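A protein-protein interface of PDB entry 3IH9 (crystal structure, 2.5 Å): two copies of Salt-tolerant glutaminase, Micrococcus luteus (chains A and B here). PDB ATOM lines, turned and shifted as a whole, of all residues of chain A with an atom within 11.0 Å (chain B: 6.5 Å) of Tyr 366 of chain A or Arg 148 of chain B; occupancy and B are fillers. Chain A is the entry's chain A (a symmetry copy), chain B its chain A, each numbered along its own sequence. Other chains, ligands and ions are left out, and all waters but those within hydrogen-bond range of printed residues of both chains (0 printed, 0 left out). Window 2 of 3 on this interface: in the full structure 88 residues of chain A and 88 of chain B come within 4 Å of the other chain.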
ATOM      1  N   THR A 359      -3.453 -24.408 -22.662  1.00  0.00           N
ATOM      2  CA  THR A 359      -3.302 -22.956 -22.769  1.00  0.00           C
ATOM      3  C   THR A 359      -2.206 -22.395 -21.860  1.00  0.00           C
ATOM      4  O   THR A 359      -1.706 -21.295 -22.091  1.00  0.00           O
ATOM      5  CB  THR A 359      -4.637 -22.227 -22.426  1.00  0.00           C
ATOM      6  OG1 THR A 359      -5.714 -22.809 -23.176  1.00  0.00           O
ATOM      7  CG2 THR A 359      -4.543 -20.735 -22.762  1.00  0.00           C
ATOM      8  N   GLY A 360      -1.834 -23.154 -20.834  1.00  0.00           N
ATOM      9  CA  GLY A 360      -0.819 -22.698 -19.905  1.00  0.00           C
ATOM     10  C   GLY A 360      -1.493 -21.829 -18.864  1.00  0.00           C
ATOM     11  O   GLY A 360      -1.209 -21.923 -17.672  1.00  0.00           O
ATOM     12  N   TRP A 361      -2.414 -20.991 -19.330  1.00  0.00           N
ATOM     13  CA  TRP A 361      -3.146 -20.081 -18.461  1.00  0.00           C
ATOM     14  C   TRP A 361      -4.658 -20.212 -18.604  1.00  0.00           C
ATOM     15  O   TRP A 361      -5.170 -20.646 -19.639  1.00  0.00           O
ATOM     16  CB  TRP A 361      -2.752 -18.636 -18.760  1.00  0.00           C
ATOM     17  CG  TRP A 361      -2.749 -18.315 -20.227  1.00  0.00           C
ATOM     18  CD1 TRP A 361      -1.775 -18.629 -21.131  1.00  0.00           C
ATOM     19  CD2 TRP A 361      -3.771 -17.632 -20.961  1.00  0.00           C
ATOM     20  NE1 TRP A 361      -2.124 -18.185 -22.380  1.00  0.00           N
ATOM     21  CE2 TRP A 361      -3.347 -17.566 -22.308  1.00  0.00           C
ATOM     22  CE3 TRP A 361      -5.005 -17.065 -20.613  1.00  0.00           C
ATOM     23  CZ2 TRP A 361      -4.109 -16.959 -23.310  1.00  0.00           C
ATOM     24  CZ3 TRP A 361      -5.765 -16.459 -21.609  1.00  0.00           C
ATOM     25  CH2 TRP A 361      -5.311 -16.412 -22.944  1.00  0.00           C
ATOM     26  N   ASP A 362      -5.361 -19.809 -17.552  1.00  0.00           N
ATOM     27  CA  ASP A 362      -6.813 -19.854 -17.522  1.00  0.00           C
ATOM     28  C   ASP A 362      -7.394 -18.603 -18.158  1.00  0.00           C
ATOM     29  O   ASP A 362      -7.211 -17.501 -17.645  1.00  0.00           O
ATOM     30  CB  ASP A 362      -7.305 -19.932 -16.080  1.00  0.00           C
ATOM     31  CG  ASP A 362      -8.806 -20.063 -15.986  1.00  0.00           C
ATOM     32  OD1 ASP A 362      -9.515 -19.558 -16.886  1.00  0.00           O
ATOM     33  OD2 ASP A 362      -9.278 -20.665 -14.999  1.00  0.00           O
ATOM     34  N   ALA A 363      -8.107 -18.784 -19.263  1.00  0.00           N
ATOM     35  CA  ALA A 363      -8.743 -17.680 -19.974  1.00  0.00           C
ATOM     36  C   ALA A 363      -9.649 -16.875 -19.045  1.00  0.00           C
ATOM     37  O   ALA A 363      -9.751 -15.658 -19.167  1.00  0.00           O
ATOM     38  CB  ALA A 363      -9.553 -18.218 -21.133  1.00  0.00           C
ATOM     39  N   ALA A 364     -10.311 -17.564 -18.121  1.00  0.00           N
ATOM     40  CA  ALA A 364     -11.204 -16.905 -17.177  1.00  0.00           C
ATOM     41  C   ALA A 364     -10.445 -15.934 -16.280  1.00  0.00           C
ATOM     42  O   ALA A 364     -10.914 -14.826 -16.007  1.00  0.00           O
ATOM     43  CB  ALA A 364     -11.912 -17.941 -16.329  1.00  0.00           C
ATOM     44  N   VAL A 365      -9.270 -16.355 -15.823  1.00  0.00           N
ATOM     45  CA  VAL A 365      -8.445 -15.529 -14.949  1.00  0.00           C
ATOM     46  C   VAL A 365      -7.746 -14.394 -15.698  1.00  0.00           C
ATOM     47  O   VAL A 365      -7.536 -13.318 -15.140  1.00  0.00           O
ATOM     48  CB  VAL A 365      -7.381 -16.385 -14.229  1.00  0.00           C
ATOM     49  CG1 VAL A 365      -6.540 -15.515 -13.308  1.00  0.00           C
ATOM     50  CG2 VAL A 365      -8.062 -17.499 -13.449  1.00  0.00           C
ATOM     51  N   TYR A 366      -7.389 -14.630 -16.958  1.00  0.00           N
ATOM     52  CA  TYR A 366      -6.714 -13.604 -17.752  1.00  0.00           C
ATOM     53  C   TYR A 366      -7.499 -13.179 -18.984  1.00  0.00           C
ATOM     54  O   TYR A 366      -7.132 -13.522 -20.104  1.00  0.00           O
ATOM     55  CB  TYR A 366      -5.337 -14.084 -18.216  1.00  0.00           C
ATOM     56  CG  TYR A 366      -4.431 -14.580 -17.120  1.00  0.00           C
ATOM     57  CD1 TYR A 366      -4.412 -15.921 -16.766  1.00  0.00           C
ATOM     58  CD2 TYR A 366      -3.576 -13.710 -16.449  1.00  0.00           C
ATOM     59  CE1 TYR A 366      -3.564 -16.390 -15.771  1.00  0.00           C
ATOM     60  CE2 TYR A 366      -2.719 -14.169 -15.447  1.00  0.00           C
ATOM     61  CZ  TYR A 366      -2.717 -15.511 -15.119  1.00  0.00           C
ATOM     62  OH  TYR A 366      -1.858 -15.978 -14.152  1.00  0.00           O
ATOM     63  N   PRO A 367      -8.585 -12.415 -18.798  1.00  0.00           N
ATOM     64  CA  PRO A 367      -9.367 -11.982 -19.959  1.00  0.00           C
ATOM     65  C   PRO A 367      -8.541 -11.215 -20.995  1.00  0.00           C
ATOM     66  O   PRO A 367      -8.731 -11.380 -22.200  1.00  0.00           O
ATOM     67  CB  PRO A 367     -10.468 -11.118 -19.332  1.00  0.00           C
ATOM     68  CG  PRO A 367      -9.827 -10.589 -18.085  1.00  0.00           C
ATOM     69  CD  PRO A 367      -9.106 -11.812 -17.560  1.00  0.00           C
ATOM     70  N   ARG A 368      -7.620 -10.383 -20.525  1.00  0.00           N
ATOM     71  CA  ARG A 368      -6.791  -9.590 -21.419  1.00  0.00           C
ATOM     72  C   ARG A 368      -5.891 -10.459 -22.283  1.00  0.00           C
ATOM     73  O   ARG A 368      -5.691 -10.172 -23.463  1.00  0.00           O
ATOM     74  CB  ARG A 368      -5.973  -8.592 -20.606  1.00  0.00           C
ATOM     75  CG  ARG A 368      -6.864  -7.661 -19.809  1.00  0.00           C
ATOM     76  CD  ARG A 368      -6.097  -6.852 -18.778  1.00  0.00           C
ATOM     77  NE  ARG A 368      -7.002  -6.156 -17.864  1.00  0.00           N
ATOM     78  CZ  ARG A 368      -7.858  -6.762 -17.042  1.00  0.00           C
ATOM     79  NH1 ARG A 368      -7.932  -8.087 -17.011  1.00  0.00           N
ATOM     80  NH2 ARG A 368      -8.642  -6.042 -16.250  1.00  0.00           N
ATOM     81  N   TRP A 369      -5.361 -11.527 -21.704  1.00  0.00           N
ATOM     82  CA  TRP A 369      -4.501 -12.432 -22.456  1.00  0.00           C
ATOM     83  C   TRP A 369      -5.276 -13.067 -23.609  1.00  0.00           C
ATOM     84  O   TRP A 369      -4.727 -13.284 -24.689  1.00  0.00           O
ATOM     85  CB  TRP A 369      -3.939 -13.509 -21.526  1.00  0.00           C
ATOM     86  CG  TRP A 369      -2.974 -12.965 -20.507  1.00  0.00           C
ATOM     87  CD1 TRP A 369      -2.813 -11.659 -20.141  1.00  0.00           C
ATOM     88  CD2 TRP A 369      -2.060 -13.720 -19.709  1.00  0.00           C
ATOM     89  NE1 TRP A 369      -1.855 -11.553 -19.162  1.00  0.00           N
ATOM     90  CE2 TRP A 369      -1.376 -12.804 -18.876  1.00  0.00           C
ATOM     91  CE3 TRP A 369      -1.754 -15.082 -19.612  1.00  0.00           C
ATOM     92  CZ2 TRP A 369      -0.399 -13.207 -17.960  1.00  0.00           C
ATOM     93  CZ3 TRP A 369      -0.782 -15.486 -18.695  1.00  0.00           C
ATOM     94  CH2 TRP A 369      -0.118 -14.548 -17.881  1.00  0.00           C
ATOM     95  N   GLN A 370      -6.555 -13.355 -23.372  1.00  0.00           N
ATOM     96  CA  GLN A 370      -7.423 -13.944 -24.394  1.00  0.00           C
ATOM     97  C   GLN A 370      -7.669 -12.932 -25.513  1.00  0.00           C
ATOM     98  O   GLN A 370      -7.521 -13.248 -26.692  1.00  0.00           O
ATOM     99  CB  GLN A 370      -8.766 -14.357 -23.779  1.00  0.00           C
ATOM    100  CG  GLN A 370      -8.726 -15.646 -22.981  1.00  0.00           C
ATOM    101  CD  GLN A 370      -9.098 -16.864 -23.813  1.00  0.00           C
ATOM    102  OE1 GLN A 370     -10.231 -16.978 -24.285  1.00  0.00           O
ATOM    103  NE2 GLN A 370      -8.148 -17.783 -23.991  1.00  0.00           N
ATOM    104  N   GLU A 371      -8.048 -11.717 -25.131  1.00  0.00           N
ATOM    105  CA  GLU A 371      -8.308 -10.666 -26.099  1.00  0.00           C
ATOM    106  C   GLU A 371      -7.098 -10.512 -27.005  1.00  0.00           C
ATOM    107  O   GLU A 371      -7.217 -10.590 -28.224  1.00  0.00           O
ATOM    108  CB  GLU A 371      -8.587  -9.343 -25.384  1.00  0.00           C
ATOM    109  CG  GLU A 371      -9.754  -9.404 -24.417  1.00  0.00           C
ATOM    110  CD  GLU A 371      -9.949  -8.108 -23.653  1.00  0.00           C
ATOM    111  OE1 GLU A 371     -10.253  -7.079 -24.292  1.00  0.00           O
ATOM    112  OE2 GLU A 371      -9.796  -8.114 -22.411  1.00  0.00           O
ATOM    113  N   ALA A 372      -5.932 -10.312 -26.400  1.00  0.00           N
ATOM    114  CA  ALA A 372      -4.695 -10.139 -27.154  1.00  0.00           C
ATOM    115  C   ALA A 372      -4.372 -11.357 -28.014  1.00  0.00           C
ATOM    116  O   ALA A 372      -3.823 -11.224 -29.107  1.00  0.00           O
ATOM    117  CB  ALA A 372      -3.540  -9.851 -26.203  1.00  0.00           C
ATOM    118  N   ALA A 373      -4.714 -12.541 -27.516  1.00  0.00           N
ATOM    119  CA  ALA A 373      -4.452 -13.773 -28.252  1.00  0.00           C
ATOM    120  C   ALA A 373      -5.328 -13.838 -29.498  1.00  0.00           C
ATOM    121  O   ALA A 373      -4.921 -14.384 -30.527  1.00  0.00           O
ATOM    122  CB  ALA A 373      -4.716 -14.981 -27.361  1.00  0.00           C
ATOM    123  N   ALA A 374      -6.528 -13.270 -29.399  1.00  0.00           N
ATOM    124  CA  ALA A 374      -7.473 -13.254 -30.508  1.00  0.00           C
ATOM    125  C   ALA A 374      -6.841 -12.676 -31.772  1.00  0.00           C
ATOM    126  O   ALA A 374      -6.884 -13.304 -32.829  1.00  0.00           O
ATOM    127  CB  ALA A 374      -8.706 -12.452 -30.124  1.00  0.00           C
ATOM    128  N   GLU B  59       1.594 -21.269  -4.699  1.00  0.00           N
ATOM    129  CA  GLU B  59       1.999 -19.950  -4.233  1.00  0.00           C
ATOM    130  C   GLU B  59       3.020 -19.938  -3.099  1.00  0.00           C
ATOM    131  O   GLU B  59       3.035 -20.819  -2.232  1.00  0.00           O
ATOM    132  CB  GLU B  59       0.781 -19.140  -3.790  1.00  0.00           C
ATOM    133  CG  GLU B  59      -0.224 -18.882  -4.885  1.00  0.00           C
ATOM    134  CD  GLU B  59      -1.258 -17.857  -4.478  1.00  0.00           C
ATOM    135  OE1 GLU B  59      -1.818 -17.994  -3.368  1.00  0.00           O
ATOM    136  OE2 GLU B  59      -1.514 -16.916  -5.268  1.00  0.00           O
ATOM    137  N   VAL B 139       2.999  -3.605  -4.733  1.00  0.00           N
ATOM    138  CA  VAL B 139       2.082  -4.654  -5.149  1.00  0.00           C
ATOM    139  C   VAL B 139       1.575  -4.422  -6.573  1.00  0.00           C
ATOM    140  O   VAL B 139       1.413  -5.375  -7.341  1.00  0.00           O
ATOM    141  CB  VAL B 139       0.864  -4.746  -4.204  1.00  0.00           C
ATOM    142  CG1 VAL B 139      -0.132  -5.757  -4.740  1.00  0.00           C
ATOM    143  CG2 VAL B 139       1.318  -5.146  -2.814  1.00  0.00           C
ATOM    144  N   MET B 142       4.317  -5.317  -9.442  1.00  0.00           N
ATOM    145  CA  MET B 142       4.468  -6.766  -9.556  1.00  0.00           C
ATOM    146  C   MET B 142       3.230  -7.400 -10.189  1.00  0.00           C
ATOM    147  O   MET B 142       3.332  -8.386 -10.928  1.00  0.00           O
ATOM    148  CB  MET B 142       4.715  -7.392  -8.178  1.00  0.00           C
ATOM    149  CG  MET B 142       6.138  -7.206  -7.660  1.00  0.00           C
ATOM    150  SD  MET B 142       6.396  -7.808  -5.976  1.00  0.00           S
ATOM    151  CE  MET B 142       6.249  -9.532  -6.250  1.00  0.00           C
ATOM    152  N   SER B 143       2.067  -6.818  -9.893  1.00  0.00           N
ATOM    153  CA  SER B 143       0.789  -7.302 -10.393  1.00  0.00           C
ATOM    154  C   SER B 143       0.583  -7.029 -11.871  1.00  0.00           C
ATOM    155  O   SER B 143       0.007  -7.857 -12.582  1.00  0.00           O
ATOM    156  CB  SER B 143      -0.354  -6.674  -9.592  1.00  0.00           C
ATOM    157  OG  SER B 143      -0.378  -7.188  -8.272  1.00  0.00           O
ATOM    158  N   LEU B 144       1.052  -5.874 -12.334  1.00  0.00           N
ATOM    159  CA  LEU B 144       0.903  -5.509 -13.740  1.00  0.00           C
ATOM    160  C   LEU B 144       1.780  -6.349 -14.654  1.00  0.00           C
ATOM    161  O   LEU B 144       1.451  -6.528 -15.825  1.00  0.00           O
ATOM    162  CB  LEU B 144       1.221  -4.022 -13.957  1.00  0.00           C
ATOM    163  CG  LEU B 144       0.215  -2.999 -13.407  1.00  0.00           C
ATOM    164  CD1 LEU B 144       0.769  -1.567 -13.533  1.00  0.00           C
ATOM    165  CD2 LEU B 144      -1.097  -3.142 -14.158  1.00  0.00           C
ATOM    166  N   LEU B 145       2.895  -6.861 -14.138  1.00  0.00           N
ATOM    167  CA  LEU B 145       3.784  -7.670 -14.964  1.00  0.00           C
ATOM    168  C   LEU B 145       3.351  -9.120 -14.877  1.00  0.00           C
ATOM    169  O   LEU B 145       3.491  -9.879 -15.837  1.00  0.00           O
ATOM    170  CB  LEU B 145       5.237  -7.524 -14.513  1.00  0.00           C
ATOM    171  CG  LEU B 145       5.822  -6.109 -14.432  1.00  0.00           C
ATOM    172  CD1 LEU B 145       7.275  -6.223 -14.008  1.00  0.00           C
ATOM    173  CD2 LEU B 145       5.716  -5.378 -15.765  1.00  0.00           C
ATOM    174  N   ALA B 146       2.817  -9.495 -13.717  1.00  0.00           N
ATOM    175  CA  ALA B 146       2.328 -10.854 -13.499  1.00  0.00           C
ATOM    176  C   ALA B 146       1.046 -11.029 -14.310  1.00  0.00           C
ATOM    177  O   ALA B 146       0.696 -12.145 -14.708  1.00  0.00           O
ATOM    178  CB  ALA B 146       2.045 -11.081 -12.019  1.00  0.00           C
ATOM    179  N   GLY B 147       0.357  -9.911 -14.549  1.00  0.00           N
ATOM    180  CA  GLY B 147      -0.886  -9.930 -15.309  1.00  0.00           C
ATOM    181  C   GLY B 147      -2.152 -10.209 -14.495  1.00  0.00           C
ATOM    182  O   GLY B 147      -3.232 -10.371 -15.065  1.00  0.00           O
ATOM    183  N   ARG B 148      -2.027 -10.266 -13.172  1.00  0.00           N
ATOM    184  CA  ARG B 148      -3.163 -10.531 -12.298  1.00  0.00           C
ATOM    185  C   ARG B 148      -2.923  -9.867 -10.954  1.00  0.00           C
ATOM    186  O   ARG B 148      -1.778  -9.669 -10.561  1.00  0.00           O
ATOM    187  CB  ARG B 148      -3.338 -12.039 -12.096  1.00  0.00           C
ATOM    188  CG  ARG B 148      -2.319 -12.700 -11.169  1.00  0.00           C
ATOM    189  CD  ARG B 148      -2.565 -14.212 -11.096  1.00  0.00           C
ATOM    190  NE  ARG B 148      -1.614 -14.931 -10.249  1.00  0.00           N
ATOM    191  CZ  ARG B 148      -1.717 -15.049  -8.929  1.00  0.00           C
ATOM    192  NH1 ARG B 148      -0.800 -15.721  -8.250  1.00  0.00           N
ATOM    193  NH2 ARG B 148      -2.743 -14.505  -8.286  1.00  0.00           N
ATOM    194  N   ARG B 149      -3.992  -9.518 -10.247  1.00  0.00           N
ATOM    195  CA  ARG B 149      -3.843  -8.889  -8.948  1.00  0.00           C
ATOM    196  C   ARG B 149      -3.248  -9.876  -7.946  1.00  0.00           C
ATOM    197  O   ARG B 149      -3.777 -10.977  -7.752  1.00  0.00           O
ATOM    198  CB  ARG B 149      -5.186  -8.366  -8.448  1.00  0.00           C
ATOM    199  CG  ARG B 149      -5.531  -6.987  -9.000  1.00  0.00           C
ATOM    200  CD  ARG B 149      -6.824  -6.424  -8.407  1.00  0.00           C
ATOM    201  NE  ARG B 149      -6.945  -4.984  -8.646  1.00  0.00           N
ATOM    202  CZ  ARG B 149      -6.238  -4.051  -8.007  1.00  0.00           C
ATOM    203  NH1 ARG B 149      -5.356  -4.399  -7.078  1.00  0.00           N
ATOM    204  NH2 ARG B 149      -6.402  -2.769  -8.304  1.00  0.00           N
ATOM    205  N   LEU B 150      -2.130  -9.479  -7.336  1.00  0.00           N
ATOM    206  CA  LEU B 150      -1.438 -10.310  -6.356  1.00  0.00           C
ATOM    207  C   LEU B 150      -1.813  -9.904  -4.943  1.00  0.00           C
ATOM    208  O   LEU B 150      -2.298  -8.802  -4.709  1.00  0.00           O
ATOM    209  CB  LEU B 150       0.079 -10.204  -6.533  1.00  0.00           C
ATOM    210  CG  LEU B 150       0.635 -10.649  -7.887  1.00  0.00           C
ATOM    211  CD1 LEU B 150       2.136 -10.415  -7.933  1.00  0.00           C
ATOM    212  CD2 LEU B 150       0.301 -12.121  -8.114  1.00  0.00           C
ATOM    213  N   SER B 151      -1.557 -10.798  -3.997  1.00  0.00           N
ATOM    214  CA  SER B 151      -1.898 -10.549  -2.609  1.00  0.00           C
ATOM    215  C   SER B 151      -0.712 -10.732  -1.675  1.00  0.00           C
ATOM    216  O   SER B 151       0.222 -11.482  -1.969  1.00  0.00           O
ATOM    217  CB  SER B 151      -3.026 -11.499  -2.185  1.00  0.00           C
ATOM    218  OG  SER B 151      -4.022 -11.592  -3.194  1.00  0.00           O
ATOM    219  N   LEU B 198       2.406 -12.907  -2.741  1.00  0.00           N
ATOM    220  CA  LEU B 198       2.314 -14.295  -3.204  1.00  0.00           C
ATOM    221  C   LEU B 198       2.321 -14.457  -4.708  1.00  0.00           C
ATOM    222  O   LEU B 198       1.526 -13.843  -5.414  1.00  0.00           O
ATOM    223  CB  LEU B 198       1.065 -14.948  -2.636  1.00  0.00           C
ATOM    224  CG  LEU B 198       1.158 -15.119  -1.122  1.00  0.00           C
ATOM    225  CD1 LEU B 198      -0.235 -15.266  -0.517  1.00  0.00           C
ATOM    226  CD2 LEU B 198       2.048 -16.316  -0.821  1.00  0.00           C
ATOM    227  N   VAL B 199       3.228 -15.300  -5.187  1.00  0.00           N
ATOM    228  CA  VAL B 199       3.376 -15.566  -6.614  1.00  0.00           C
ATOM    229  C   VAL B 199       3.661 -17.043  -6.831  1.00  0.00           C
ATOM    230  O   VAL B 199       4.024 -17.768  -5.899  1.00  0.00           O
ATOM    231  CB  VAL B 199       4.572 -14.773  -7.240  1.00  0.00           C
ATOM    232  CG1 VAL B 199       4.412 -13.279  -7.011  1.00  0.00           C
ATOM    233  CG2 VAL B 199       5.893 -15.273  -6.662  1.00  0.00           C
ATOM    234  N   THR B 200       3.508 -17.481  -8.070  1.00  0.00           N
ATOM    235  CA  THR B 200       3.784 -18.863  -8.408  1.00  0.00           C
ATOM    236  C   THR B 200       4.946 -18.874  -9.386  1.00  0.00           C
ATOM    237  O   THR B 200       5.325 -17.842  -9.928  1.00  0.00           O
ATOM    238  CB  THR B 200       2.610 -19.515  -9.107  1.00  0.00           C
ATOM    239  OG1 THR B 200       2.475 -18.945 -10.414  1.00  0.00           O
ATOM    240  CG2 THR B 200       1.333 -19.313  -8.305  1.00  0.00           C
ATOM    241  N   LYS B 202       4.969 -19.699 -12.267  1.00  0.00           N
ATOM    242  CA  LYS B 202       4.480 -19.136 -13.517  1.00  0.00           C
ATOM    243  C   LYS B 202       4.450 -17.623 -13.494  1.00  0.00           C
ATOM    244  O   LYS B 202       4.835 -16.990 -14.475  1.00  0.00           O
ATOM    245  CB  LYS B 202       3.086 -19.670 -13.838  1.00  0.00           C
ATOM    246  CG  LYS B 202       3.069 -21.126 -14.255  1.00  0.00           C
ATOM    247  CD  LYS B 202       1.653 -21.594 -14.523  1.00  0.00           C
ATOM    248  CE  LYS B 202       1.629 -23.049 -14.923  1.00  0.00           C
ATOM    249  NZ  LYS B 202       0.238 -23.563 -15.056  1.00  0.00           N
ATOM    250  N   ASP B 203       3.989 -17.048 -12.382  1.00  0.00           N
ATOM    251  CA  ASP B 203       3.943 -15.595 -12.229  1.00  0.00           C
ATOM    252  C   ASP B 203       5.338 -15.011 -12.466  1.00  0.00           C
ATOM    253  O   ASP B 203       5.503 -14.063 -13.235  1.00  0.00           O
ATOM    254  CB  ASP B 203       3.472 -15.202 -10.817  1.00  0.00           C
ATOM    255  CG  ASP B 203       2.003 -15.537 -10.558  1.00  0.00           C
ATOM    256  OD1 ASP B 203       1.132 -15.163 -11.373  1.00  0.00           O
ATOM    257  OD2 ASP B 203       1.718 -16.165  -9.518  1.00  0.00           O
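No position is printed for both chains.
Of the 4 pairs that touch across the chains among the printed residues, none has its exchanged pair printed and touching as well.
Among the printed residues, pairs that only touch across the chains: Trp 369 of chain A with Ala 146 of chain B (3.6 Å), Tyr 366 of chain A with Arg 148 of chain B (3.6 Å) and Tyr 366 of chain A with Gly 147 of chain B (3.6 Å).
Of the 16 printed residues of chain A, 3 touch a printed residue of chain B.
Hydrophobic or aromatic side chains of chain A within 4 Å of the printed part of chain B: Tyr 366 and Trp 369.
The guanidinium group (NH1) of Arg 148 of chain B lies within salt-bridge range of the side-chain carboxylate (OE2) of Glu 59 of chain B, 3.3 Å away.
O of Ser 143 of chain B sits at hydrogen-bond distance from N of Arg 148 of chain B (3.2 Å).
NH1 of Arg 148 of chain B is in salt-bridge range of OD2 of Asp 203 of chain B (2.9 Å).
The backbone NH of Lys 202 of chain B sits close to the side-chain hydroxyl of Thr 200 of chain B, at 3.2 Å.
Printed residues of chain B within 4 Å of Gly 360 of chain A: Lys 202.
Of chain B, only Gly 147 (3.6 Å) and Arg 148 (3.6 Å) come within 4 Å of Tyr 366 of chain A.
Of the printed residues of chain B, Trp 369 of chain A touches Ala 146 (3.6 Å).
Ser 143 of chain B touches none of the printed residues of chain A.
Of the printed residues of chain A, Ala 146 of chain B touches Trp 369 (3.6 Å).
Gly 147 of chain B touches one residue of chain A.
Arg 148 of chain B touches just one residue of chain A: Tyr 366 (3.6 Å).
No residue of chain A comes within 4 Å of Leu 150 of chain B.
No residue of chain A comes within 4 Å of Val 199 of chain B.
No residue of chain A comes within 4 Å of Thr 200 of chain B.
Printed residues of chain A within 4 Å of Lys 202 of chain B: Gly 360.
The nearest residue of chain B that does not touch Tyr 366 of chain A is Ala 146 of chain B (4.04 Å).
The nearest residue of chain A that does not touch Arg 148 of chain B is Val 365 of chain A (4.7 Å).
The nearest printed residue of chain B that does not touch Gly 360 of chain A is Thr 200 of chain B (8.7 Å).
O of Gly 360 of chain A sits at hydrogen-bond distance from NZ of Lys 202 of chain B (3.4 Å).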
